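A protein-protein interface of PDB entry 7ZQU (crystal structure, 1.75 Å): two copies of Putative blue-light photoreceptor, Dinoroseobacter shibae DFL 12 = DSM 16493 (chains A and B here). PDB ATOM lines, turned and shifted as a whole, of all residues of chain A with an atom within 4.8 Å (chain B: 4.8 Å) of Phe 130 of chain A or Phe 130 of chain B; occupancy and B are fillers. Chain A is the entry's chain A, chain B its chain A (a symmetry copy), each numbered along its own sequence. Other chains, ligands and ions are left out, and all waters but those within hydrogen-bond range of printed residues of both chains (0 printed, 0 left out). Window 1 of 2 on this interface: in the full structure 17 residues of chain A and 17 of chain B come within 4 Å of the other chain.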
ATOM      1  N   LEU A  24      14.281 -14.482 -21.023  1.00  0.00           N
ATOM      2  CA  LEU A  24      14.105 -15.122 -22.321  1.00  0.00           C
ATOM      3  C   LEU A  24      14.423 -16.616 -22.295  1.00  0.00           C
ATOM      4  O   LEU A  24      14.087 -17.318 -23.255  1.00  0.00           O
ATOM      5  CB  LEU A  24      14.959 -14.409 -23.373  1.00  0.00           C
ATOM      6  CG  LEU A  24      14.228 -13.300 -24.136  1.00  0.00           C
ATOM      7  CD1 LEU A  24      14.055 -12.062 -23.271  1.00  0.00           C
ATOM      8  CD2 LEU A  24      14.960 -12.971 -25.418  1.00  0.00           C
ATOM      9  N   LEU A  27      11.716 -19.020 -23.169  1.00  0.00           N
ATOM     10  CA  LEU A  27      11.404 -19.420 -24.534  1.00  0.00           C
ATOM     11  C   LEU A  27      12.001 -20.773 -24.896  1.00  0.00           C
ATOM     12  O   LEU A  27      11.575 -21.384 -25.886  1.00  0.00           O
ATOM     13  CB  LEU A  27      11.903 -18.361 -25.514  1.00  0.00           C
ATOM     14  CG  LEU A  27      11.476 -16.926 -25.197  1.00  0.00           C
ATOM     15  CD1 LEU A  27      12.069 -15.942 -26.191  1.00  0.00           C
ATOM     16  CD2 LEU A  27       9.966 -16.835 -25.168  1.00  0.00           C
ATOM     17  N   PHE A  39      20.891 -14.574 -25.760  1.00  0.00           N
ATOM     18  CA  PHE A  39      20.029 -14.540 -26.934  1.00  0.00           C
ATOM     19  C   PHE A  39      20.474 -13.396 -27.833  1.00  0.00           C
ATOM     20  O   PHE A  39      20.686 -12.280 -27.357  1.00  0.00           O
ATOM     21  CB  PHE A  39      18.555 -14.364 -26.540  1.00  0.00           C
ATOM     22  CG  PHE A  39      17.942 -15.595 -25.924  1.00  0.00           C
ATOM     23  CD1 PHE A  39      18.297 -15.983 -24.647  1.00  0.00           C
ATOM     24  CD2 PHE A  39      17.019 -16.359 -26.618  1.00  0.00           C
ATOM     25  CE1 PHE A  39      17.751 -17.124 -24.068  1.00  0.00           C
ATOM     26  CE2 PHE A  39      16.460 -17.503 -26.033  1.00  0.00           C
ATOM     27  CZ  PHE A  39      16.837 -17.870 -24.749  1.00  0.00           C
ATOM     28  N   SER A  40      20.599 -13.662 -29.130  1.00  0.00           N
ATOM     29  CA  SER A  40      21.035 -12.649 -30.073  1.00  0.00           C
ATOM     30  C   SER A  40      19.948 -12.397 -31.109  1.00  0.00           C
ATOM     31  O   SER A  40      19.081 -13.247 -31.353  1.00  0.00           O
ATOM     32  CB  SER A  40      22.325 -13.067 -30.775  1.00  0.00           C
ATOM     33  OG  SER A  40      22.019 -14.014 -31.785  1.00  0.00           O
ATOM     34  N   PRO A  42      19.643 -11.740 -34.958  1.00  0.00           N
ATOM     35  CA  PRO A  42      20.363 -11.682 -36.243  1.00  0.00           C
ATOM     36  C   PRO A  42      19.834 -10.630 -37.208  1.00  0.00           C
ATOM     37  O   PRO A  42      20.503 -10.342 -38.212  1.00  0.00           O
ATOM     38  CB  PRO A  42      20.188 -13.097 -36.806  1.00  0.00           C
ATOM     39  CG  PRO A  42      18.959 -13.625 -36.135  1.00  0.00           C
ATOM     40  CD  PRO A  42      18.932 -13.014 -34.762  1.00  0.00           C
ATOM     41  N   ILE A  50      20.702  -9.510 -27.137  1.00  0.00           N
ATOM     42  CA  ILE A  50      19.603  -8.693 -26.625  1.00  0.00           C
ATOM     43  C   ILE A  50      19.173  -9.110 -25.235  1.00  0.00           C
ATOM     44  O   ILE A  50      18.389  -8.388 -24.598  1.00  0.00           O
ATOM     45  CB  ILE A  50      18.383  -8.720 -27.571  1.00  0.00           C
ATOM     46  CG1 ILE A  50      17.962 -10.172 -27.832  1.00  0.00           C
ATOM     47  CG2 ILE A  50      18.696  -7.959 -28.857  1.00  0.00           C
ATOM     48  CD1 ILE A  50      16.546 -10.341 -28.402  1.00  0.00           C
ATOM     49  N   ARG A 119      21.421 -22.875 -30.597  1.00  0.00           N
ATOM     50  CA  ARG A 119      20.240 -23.369 -31.310  1.00  0.00           C
ATOM     51  C   ARG A 119      19.420 -22.185 -31.808  1.00  0.00           C
ATOM     52  O   ARG A 119      19.302 -21.164 -31.108  1.00  0.00           O
ATOM     53  CB  ARG A 119      19.372 -24.277 -30.423  1.00  0.00           C
ATOM     54  CG  ARG A 119      18.494 -23.538 -29.429  1.00  0.00           C
ATOM     55  N   PRO A 120      18.874 -22.268 -33.013  1.00  0.00           N
ATOM     56  CA  PRO A 120      17.929 -21.238 -33.449  1.00  0.00           C
ATOM     57  C   PRO A 120      16.646 -21.322 -32.637  1.00  0.00           C
ATOM     58  O   PRO A 120      16.235 -22.402 -32.205  1.00  0.00           O
ATOM     59  CB  PRO A 120      17.680 -21.584 -34.921  1.00  0.00           C
ATOM     60  CG  PRO A 120      17.950 -23.057 -35.013  1.00  0.00           C
ATOM     61  CD  PRO A 120      19.060 -23.326 -34.029  1.00  0.00           C
ATOM     62  N   ILE A 121      16.008 -20.168 -32.444  1.00  0.00           N
ATOM     63  CA  ILE A 121      14.702 -20.068 -31.803  1.00  0.00           C
ATOM     64  C   ILE A 121      13.716 -19.618 -32.866  1.00  0.00           C
ATOM     65  O   ILE A 121      13.879 -18.538 -33.444  1.00  0.00           O
ATOM     66  CB  ILE A 121      14.703 -19.076 -30.628  1.00  0.00           C
ATOM     67  CG1 ILE A 121      15.786 -19.447 -29.611  1.00  0.00           C
ATOM     68  CG2 ILE A 121      13.342 -19.058 -29.975  1.00  0.00           C
ATOM     69  CD1 ILE A 121      15.538 -20.769 -28.931  1.00  0.00           C
ATOM     70  N   LEU A 128      13.150 -17.792 -38.360  1.00  0.00           N
ATOM     71  CA  LEU A 128      14.147 -17.540 -37.327  1.00  0.00           C
ATOM     72  C   LEU A 128      13.798 -16.273 -36.554  1.00  0.00           C
ATOM     73  O   LEU A 128      13.596 -15.209 -37.151  1.00  0.00           O
ATOM     74  CB  LEU A 128      15.521 -17.408 -37.968  1.00  0.00           C
ATOM     75  CG  LEU A 128      16.704 -17.207 -37.023  1.00  0.00           C
ATOM     76  CD1 LEU A 128      16.892 -18.464 -36.220  1.00  0.00           C
ATOM     77  CD2 LEU A 128      17.951 -16.879 -37.812  1.00  0.00           C
ATOM     78  N   MET A 129      13.712 -16.389 -35.226  1.00  0.00           N
ATOM     79  CA  MET A 129      13.485 -15.245 -34.345  1.00  0.00           C
ATOM     80  C   MET A 129      14.783 -14.794 -33.694  1.00  0.00           C
ATOM     81  O   MET A 129      15.194 -13.639 -33.839  1.00  0.00           O
ATOM     82  CB  MET A 129      12.507 -15.567 -33.203  1.00  0.00           C
ATOM     83  CG  MET A 129      11.101 -15.929 -33.550  1.00  0.00           C
ATOM     84  SD  MET A 129      10.056 -15.763 -32.075  1.00  0.00           S
ATOM     85  CE  MET A 129      10.070 -14.002 -31.874  1.00  0.00           C
ATOM     86  N   PHE A 130      15.405 -15.699 -32.940  1.00  0.00           N
ATOM     87  CA  PHE A 130      16.630 -15.438 -32.206  1.00  0.00           C
ATOM     88  C   PHE A 130      17.550 -16.638 -32.342  1.00  0.00           C
ATOM     89  O   PHE A 130      17.130 -17.735 -32.727  1.00  0.00           O
ATOM     90  CB  PHE A 130      16.375 -15.208 -30.708  1.00  0.00           C
ATOM     91  CG  PHE A 130      15.196 -14.346 -30.407  1.00  0.00           C
ATOM     92  CD1 PHE A 130      15.202 -13.004 -30.743  1.00  0.00           C
ATOM     93  CD2 PHE A 130      14.100 -14.864 -29.741  1.00  0.00           C
ATOM     94  CE1 PHE A 130      14.127 -12.191 -30.446  1.00  0.00           C
ATOM     95  CE2 PHE A 130      13.016 -14.064 -29.446  1.00  0.00           C
ATOM     96  CZ  PHE A 130      13.030 -12.715 -29.792  1.00  0.00           C
ATOM     97  N   PHE A 131      18.811 -16.435 -31.979  1.00  0.00           N
ATOM     98  CA  PHE A 131      19.698 -17.529 -31.607  1.00  0.00           C
ATOM     99  C   PHE A 131      19.831 -17.557 -30.093  1.00  0.00           C
ATOM    100  O   PHE A 131      19.926 -16.505 -29.452  1.00  0.00           O
ATOM    101  CB  PHE A 131      21.079 -17.378 -32.235  1.00  0.00           C
ATOM    102  CG  PHE A 131      21.106 -17.582 -33.729  1.00  0.00           C
ATOM    103  CD1 PHE A 131      21.003 -18.855 -34.270  1.00  0.00           C
ATOM    104  CD2 PHE A 131      21.276 -16.503 -34.587  1.00  0.00           C
ATOM    105  CE1 PHE A 131      21.037 -19.054 -35.657  1.00  0.00           C
ATOM    106  CE2 PHE A 131      21.310 -16.690 -35.972  1.00  0.00           C
ATOM    107  CZ  PHE A 131      21.189 -17.971 -36.509  1.00  0.00           C
ATOM    108  N   ALA A 132      19.826 -18.760 -29.523  1.00  0.00           N
ATOM    109  CA  ALA A 132      20.189 -18.970 -28.128  1.00  0.00           C
ATOM    110  C   ALA A 132      21.551 -19.648 -28.075  1.00  0.00           C
ATOM    111  O   ALA A 132      21.828 -20.552 -28.864  1.00  0.00           O
ATOM    112  CB  ALA A 132      19.150 -19.827 -27.403  1.00  0.00           C
ATOM    113  N   LEU B  24       6.217 -16.114 -26.129  1.00  0.00           N
ATOM    114  CA  LEU B  24       6.767 -14.866 -25.614  1.00  0.00           C
ATOM    115  C   LEU B  24       5.910 -14.250 -24.509  1.00  0.00           C
ATOM    116  O   LEU B  24       6.380 -13.331 -23.828  1.00  0.00           O
ATOM    117  CB  LEU B  24       6.960 -13.871 -26.762  1.00  0.00           C
ATOM    118  CG  LEU B  24       8.355 -13.897 -27.394  1.00  0.00           C
ATOM    119  CD1 LEU B  24       8.535 -15.122 -28.275  1.00  0.00           C
ATOM    120  CD2 LEU B  24       8.605 -12.625 -28.174  1.00  0.00           C
ATOM    121  N   LEU B  27       7.430 -13.781 -21.142  1.00  0.00           N
ATOM    122  CA  LEU B  27       8.214 -12.613 -20.767  1.00  0.00           C
ATOM    123  C   LEU B  27       7.407 -11.602 -19.963  1.00  0.00           C
ATOM    124  O   LEU B  27       7.995 -10.726 -19.315  1.00  0.00           O
ATOM    125  CB  LEU B  27       8.776 -11.941 -22.018  1.00  0.00           C
ATOM    126  CG  LEU B  27       9.513 -12.871 -22.983  1.00  0.00           C
ATOM    127  CD1 LEU B  27       9.981 -12.123 -24.221  1.00  0.00           C
ATOM    128  CD2 LEU B  27      10.670 -13.537 -22.272  1.00  0.00           C
ATOM    129  N   PHE B  39       3.673  -9.392 -29.933  1.00  0.00           N
ATOM    130  CA  PHE B  39       4.946  -8.755 -29.622  1.00  0.00           C
ATOM    131  C   PHE B  39       5.541  -8.202 -30.908  1.00  0.00           C
ATOM    132  O   PHE B  39       5.585  -8.900 -31.921  1.00  0.00           O
ATOM    133  CB  PHE B  39       5.922  -9.744 -28.967  1.00  0.00           C
ATOM    134  CG  PHE B  39       5.565 -10.095 -27.546  1.00  0.00           C
ATOM    135  CD1 PHE B  39       4.476 -10.904 -27.282  1.00  0.00           C
ATOM    136  CD2 PHE B  39       6.311  -9.618 -26.482  1.00  0.00           C
ATOM    137  CE1 PHE B  39       4.125 -11.227 -25.976  1.00  0.00           C
ATOM    138  CE2 PHE B  39       5.965  -9.951 -25.166  1.00  0.00           C
ATOM    139  CZ  PHE B  39       4.865 -10.763 -24.931  1.00  0.00           C
ATOM    140  N   SER B  40       6.014  -6.960 -30.869  1.00  0.00           N
ATOM    141  CA  SER B  40       6.587  -6.329 -32.043  1.00  0.00           C
ATOM    142  C   SER B  40       8.046  -5.974 -31.789  1.00  0.00           C
ATOM    143  O   SER B  40       8.482  -5.827 -30.638  1.00  0.00           O
ATOM    144  CB  SER B  40       5.813  -5.069 -32.426  1.00  0.00           C
ATOM    145  OG  SER B  40       6.185  -4.012 -31.557  1.00  0.00           O
ATOM    146  N   PRO B  42      10.543  -3.055 -32.546  1.00  0.00           N
ATOM    147  CA  PRO B  42      10.694  -1.693 -33.090  1.00  0.00           C
ATOM    148  C   PRO B  42      12.020  -1.446 -33.798  1.00  0.00           C
ATOM    149  O   PRO B  42      12.155  -0.422 -34.484  1.00  0.00           O
ATOM    150  CB  PRO B  42      10.547  -0.803 -31.850  1.00  0.00           C
ATOM    151  CG  PRO B  42      10.908  -1.689 -30.700  1.00  0.00           C
ATOM    152  CD  PRO B  42      10.462  -3.074 -31.077  1.00  0.00           C
ATOM    153  N   ILE B  50       6.578 -10.026 -34.261  1.00  0.00           N
ATOM    154  CA  ILE B  50       7.468 -11.183 -34.334  1.00  0.00           C
ATOM    155  C   ILE B  50       6.900 -12.395 -33.627  1.00  0.00           C
ATOM    156  O   ILE B  50       7.450 -13.498 -33.773  1.00  0.00           O
ATOM    157  CB  ILE B  50       8.867 -10.863 -33.765  1.00  0.00           C
ATOM    158  CG1 ILE B  50       8.734 -10.317 -32.338  1.00  0.00           C
ATOM    159  CG2 ILE B  50       9.608  -9.905 -34.693  1.00  0.00           C
ATOM    160  CD1 ILE B  50      10.026 -10.347 -31.511  1.00  0.00           C
ATOM    161  N   ARG B 119       2.438  -2.241 -23.614  1.00  0.00           N
ATOM    162  CA  ARG B 119       3.498  -1.944 -22.646  1.00  0.00           C
ATOM    163  C   ARG B 119       4.853  -2.257 -23.270  1.00  0.00           C
ATOM    164  O   ARG B 119       4.989  -3.247 -24.010  1.00  0.00           O
ATOM    165  CB  ARG B 119       3.322  -2.738 -21.340  1.00  0.00           C
ATOM    166  CG  ARG B 119       3.764  -4.189 -21.418  1.00  0.00           C
ATOM    167  N   PRO B 120       5.857  -1.426 -23.028  1.00  0.00           N
ATOM    168  CA  PRO B 120       7.211  -1.790 -23.452  1.00  0.00           C
ATOM    169  C   PRO B 120       7.718  -2.968 -22.637  1.00  0.00           C
ATOM    170  O   PRO B 120       7.367  -3.132 -21.466  1.00  0.00           O
ATOM    171  CB  PRO B 120       8.024  -0.522 -23.165  1.00  0.00           C
ATOM    172  CG  PRO B 120       7.274   0.167 -22.065  1.00  0.00           C
ATOM    173  CD  PRO B 120       5.817  -0.128 -22.322  1.00  0.00           C
ATOM    174  N   ILE B 121       8.564  -3.783 -23.266  1.00  0.00           N
ATOM    175  CA  ILE B 121       9.254  -4.889 -22.612  1.00  0.00           C
ATOM    176  C   ILE B 121      10.731  -4.539 -22.580  1.00  0.00           C
ATOM    177  O   ILE B 121      11.345  -4.350 -23.635  1.00  0.00           O
ATOM    178  CB  ILE B 121       9.043  -6.224 -23.344  1.00  0.00           C
ATOM    179  CG1 ILE B 121       7.549  -6.524 -23.498  1.00  0.00           C
ATOM    180  CG2 ILE B 121       9.734  -7.335 -22.590  1.00  0.00           C
ATOM    181  CD1 ILE B 121       6.847  -6.750 -22.183  1.00  0.00           C
ATOM    182  N   LEU B 128      14.754  -0.727 -24.348  1.00  0.00           N
ATOM    183  CA  LEU B 128      13.568  -1.286 -24.984  1.00  0.00           C
ATOM    184  C   LEU B 128      13.939  -2.516 -25.806  1.00  0.00           C
ATOM    185  O   LEU B 128      14.832  -2.454 -26.660  1.00  0.00           O
ATOM    186  CB  LEU B 128      12.921  -0.233 -25.871  1.00  0.00           C
ATOM    187  CG  LEU B 128      11.621  -0.626 -26.569  1.00  0.00           C
ATOM    188  CD1 LEU B 128      10.554  -0.802 -25.524  1.00  0.00           C
ATOM    189  CD2 LEU B 128      11.224   0.437 -27.571  1.00  0.00           C
ATOM    190  N   MET B 129      13.267  -3.639 -25.539  1.00  0.00           N
ATOM    191  CA  MET B 129      13.441  -4.868 -26.309  1.00  0.00           C
ATOM    192  C   MET B 129      12.308  -5.049 -27.306  1.00  0.00           C
ATOM    193  O   MET B 129      12.541  -5.155 -28.515  1.00  0.00           O
ATOM    194  CB  MET B 129      13.452  -6.122 -25.420  1.00  0.00           C
ATOM    195  CG  MET B 129      14.545  -6.273 -24.414  1.00  0.00           C
ATOM    196  SD  MET B 129      14.629  -8.003 -23.873  1.00  0.00           S
ATOM    197  CE  MET B 129      15.226  -8.769 -25.356  1.00  0.00           C
ATOM    198  N   PHE B 130      11.082  -5.129 -26.792  1.00  0.00           N
ATOM    199  CA  PHE B 130       9.884  -5.347 -27.583  1.00  0.00           C
ATOM    200  C   PHE B 130       8.778  -4.451 -27.056  1.00  0.00           C
ATOM    201  O   PHE B 130       8.851  -3.919 -25.942  1.00  0.00           O
ATOM    202  CB  PHE B 130       9.389  -6.800 -27.505  1.00  0.00           C
ATOM    203  CG  PHE B 130      10.467  -7.825 -27.596  1.00  0.00           C
ATOM    204  CD1 PHE B 130      11.180  -7.996 -28.769  1.00  0.00           C
ATOM    205  CD2 PHE B 130      10.736  -8.657 -26.523  1.00  0.00           C
ATOM    206  CE1 PHE B 130      12.163  -8.960 -28.872  1.00  0.00           C
ATOM    207  CE2 PHE B 130      11.721  -9.618 -26.610  1.00  0.00           C
ATOM    208  CZ  PHE B 130      12.436  -9.777 -27.795  1.00  0.00           C
ATOM    209  N   PHE B 131       7.722  -4.318 -27.851  1.00  0.00           N
ATOM    210  CA  PHE B 131       6.420  -3.903 -27.349  1.00  0.00           C
ATOM    211  C   PHE B 131       5.520  -5.125 -27.253  1.00  0.00           C
ATOM    212  O   PHE B 131       5.540  -5.989 -28.136  1.00  0.00           O
ATOM    213  CB  PHE B 131       5.769  -2.863 -28.254  1.00  0.00           C
ATOM    214  CG  PHE B 131       6.443  -1.514 -28.234  1.00  0.00           C
ATOM    215  CD1 PHE B 131       6.287  -0.662 -27.150  1.00  0.00           C
ATOM    216  CD2 PHE B 131       7.197  -1.086 -29.319  1.00  0.00           C
ATOM    217  CE1 PHE B 131       6.903   0.596 -27.128  1.00  0.00           C
ATOM    218  CE2 PHE B 131       7.818   0.168 -29.306  1.00  0.00           C
ATOM    219  CZ  PHE B 131       7.671   1.011 -28.207  1.00  0.00           C
ATOM    220  N   ALA B 132       4.741  -5.200 -26.176  1.00  0.00           N
ATOM    221  CA  ALA B 132       3.657  -6.166 -26.056  1.00  0.00           C
ATOM    222  C   ALA B 132       2.331  -5.430 -26.185  1.00  0.00           C
ATOM    223  O   ALA B 132       2.168  -4.339 -25.635  1.00  0.00           O
ATOM    224  CB  ALA B 132       3.716  -6.910 -24.720  1.00  0.00           C
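The backbone carbonyl oxygen (O) of Phe 39 of chain A sits at hydrogen-bond distance from the backbone NH (N) of Ile 50 of chain A.
O of Ile 121 of chain A sits at hydrogen-bond distance from N of Met 129 of chain A.
The backbone NH of Ile 121 of chain A sits at hydrogen-bond distance from the backbone carbonyl oxygen of Phe 130 of chain A (2.7 Å).
The backbone carbonyl oxygen (O) of Phe 130 of chain B is in hydrogen-bond range of the backbone NH (N) of Ile 121 of chain B, 2.7 Å away.
The backbone NH (N) of Met 129 of chain B lies within hydrogen-bond range of the backbone carbonyl oxygen (O) of Ile 121 of chain B, at 2.8 Å.
The backbone carbonyl oxygen (O) of Phe 39 of chain B is in hydrogen-bond range of the backbone NH (N) of Ile 50 of chain B, 2.8 Å away.
Among the printed residues, merely in contact across the chains: Leu 24 of chain A with Leu 27 of chain B, Leu 27 of chain A with Leu 24 of chain B, Ile 50 of chain A with Met 129 of chain B, Met 129 of chain A with Ile 50 of chain B and Phe 130 of chain A with Phe 130 of chain B.
Phe 130 of chain B touches just one residue of chain A: Phe 130.
Of the printed residues of chain B, Leu 24 of chain A touches Leu 27.
Printed residues of chain A within 4 Å of Ile 50 of chain B: Met 129.
The nearest residue of chain A that does not touch Phe 130 of chain B is Ile 50 of chain A (4.2 Å).
Of the 14 printed residues of chain B, 5 touch a printed residue of chain A.
Printed residues of chain B that touch a printed residue of chain A: Leu 24, Leu 27, Ile 50, Met 129 and Phe 130.
Hydrophobic or aromatic side chains of chain B that line the printed part of chain A: Leu 24, Leu 27, Ile 50, Met 129 and Phe 130.
Hydrophobic or aromatic side chains of chain A that line the printed part of chain B: Leu 24, Leu 27, Ile 50, Met 129 and Phe 130.
Among the printed residues, no Asp or Glu carboxylate lies within 4 Å of a Lys or Arg side-chain nitrogen of the other chain.
Leu 24 of chain A touches Leu 27 of chain B, and with the chains exchanged Leu 27 of chain A touches Leu 24 of chain B.
Ile 50 of chain A touches Met 129 of chain B, and with the chains exchanged Met 129 of chain A touches Ile 50 of chain B.
Phe 130 of chain B touches its own counterpart, Phe 130 of chain A.
Of the 5 pairs that touch across the chains among the printed residues, 5 have their exchanged pair printed and touching as well.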
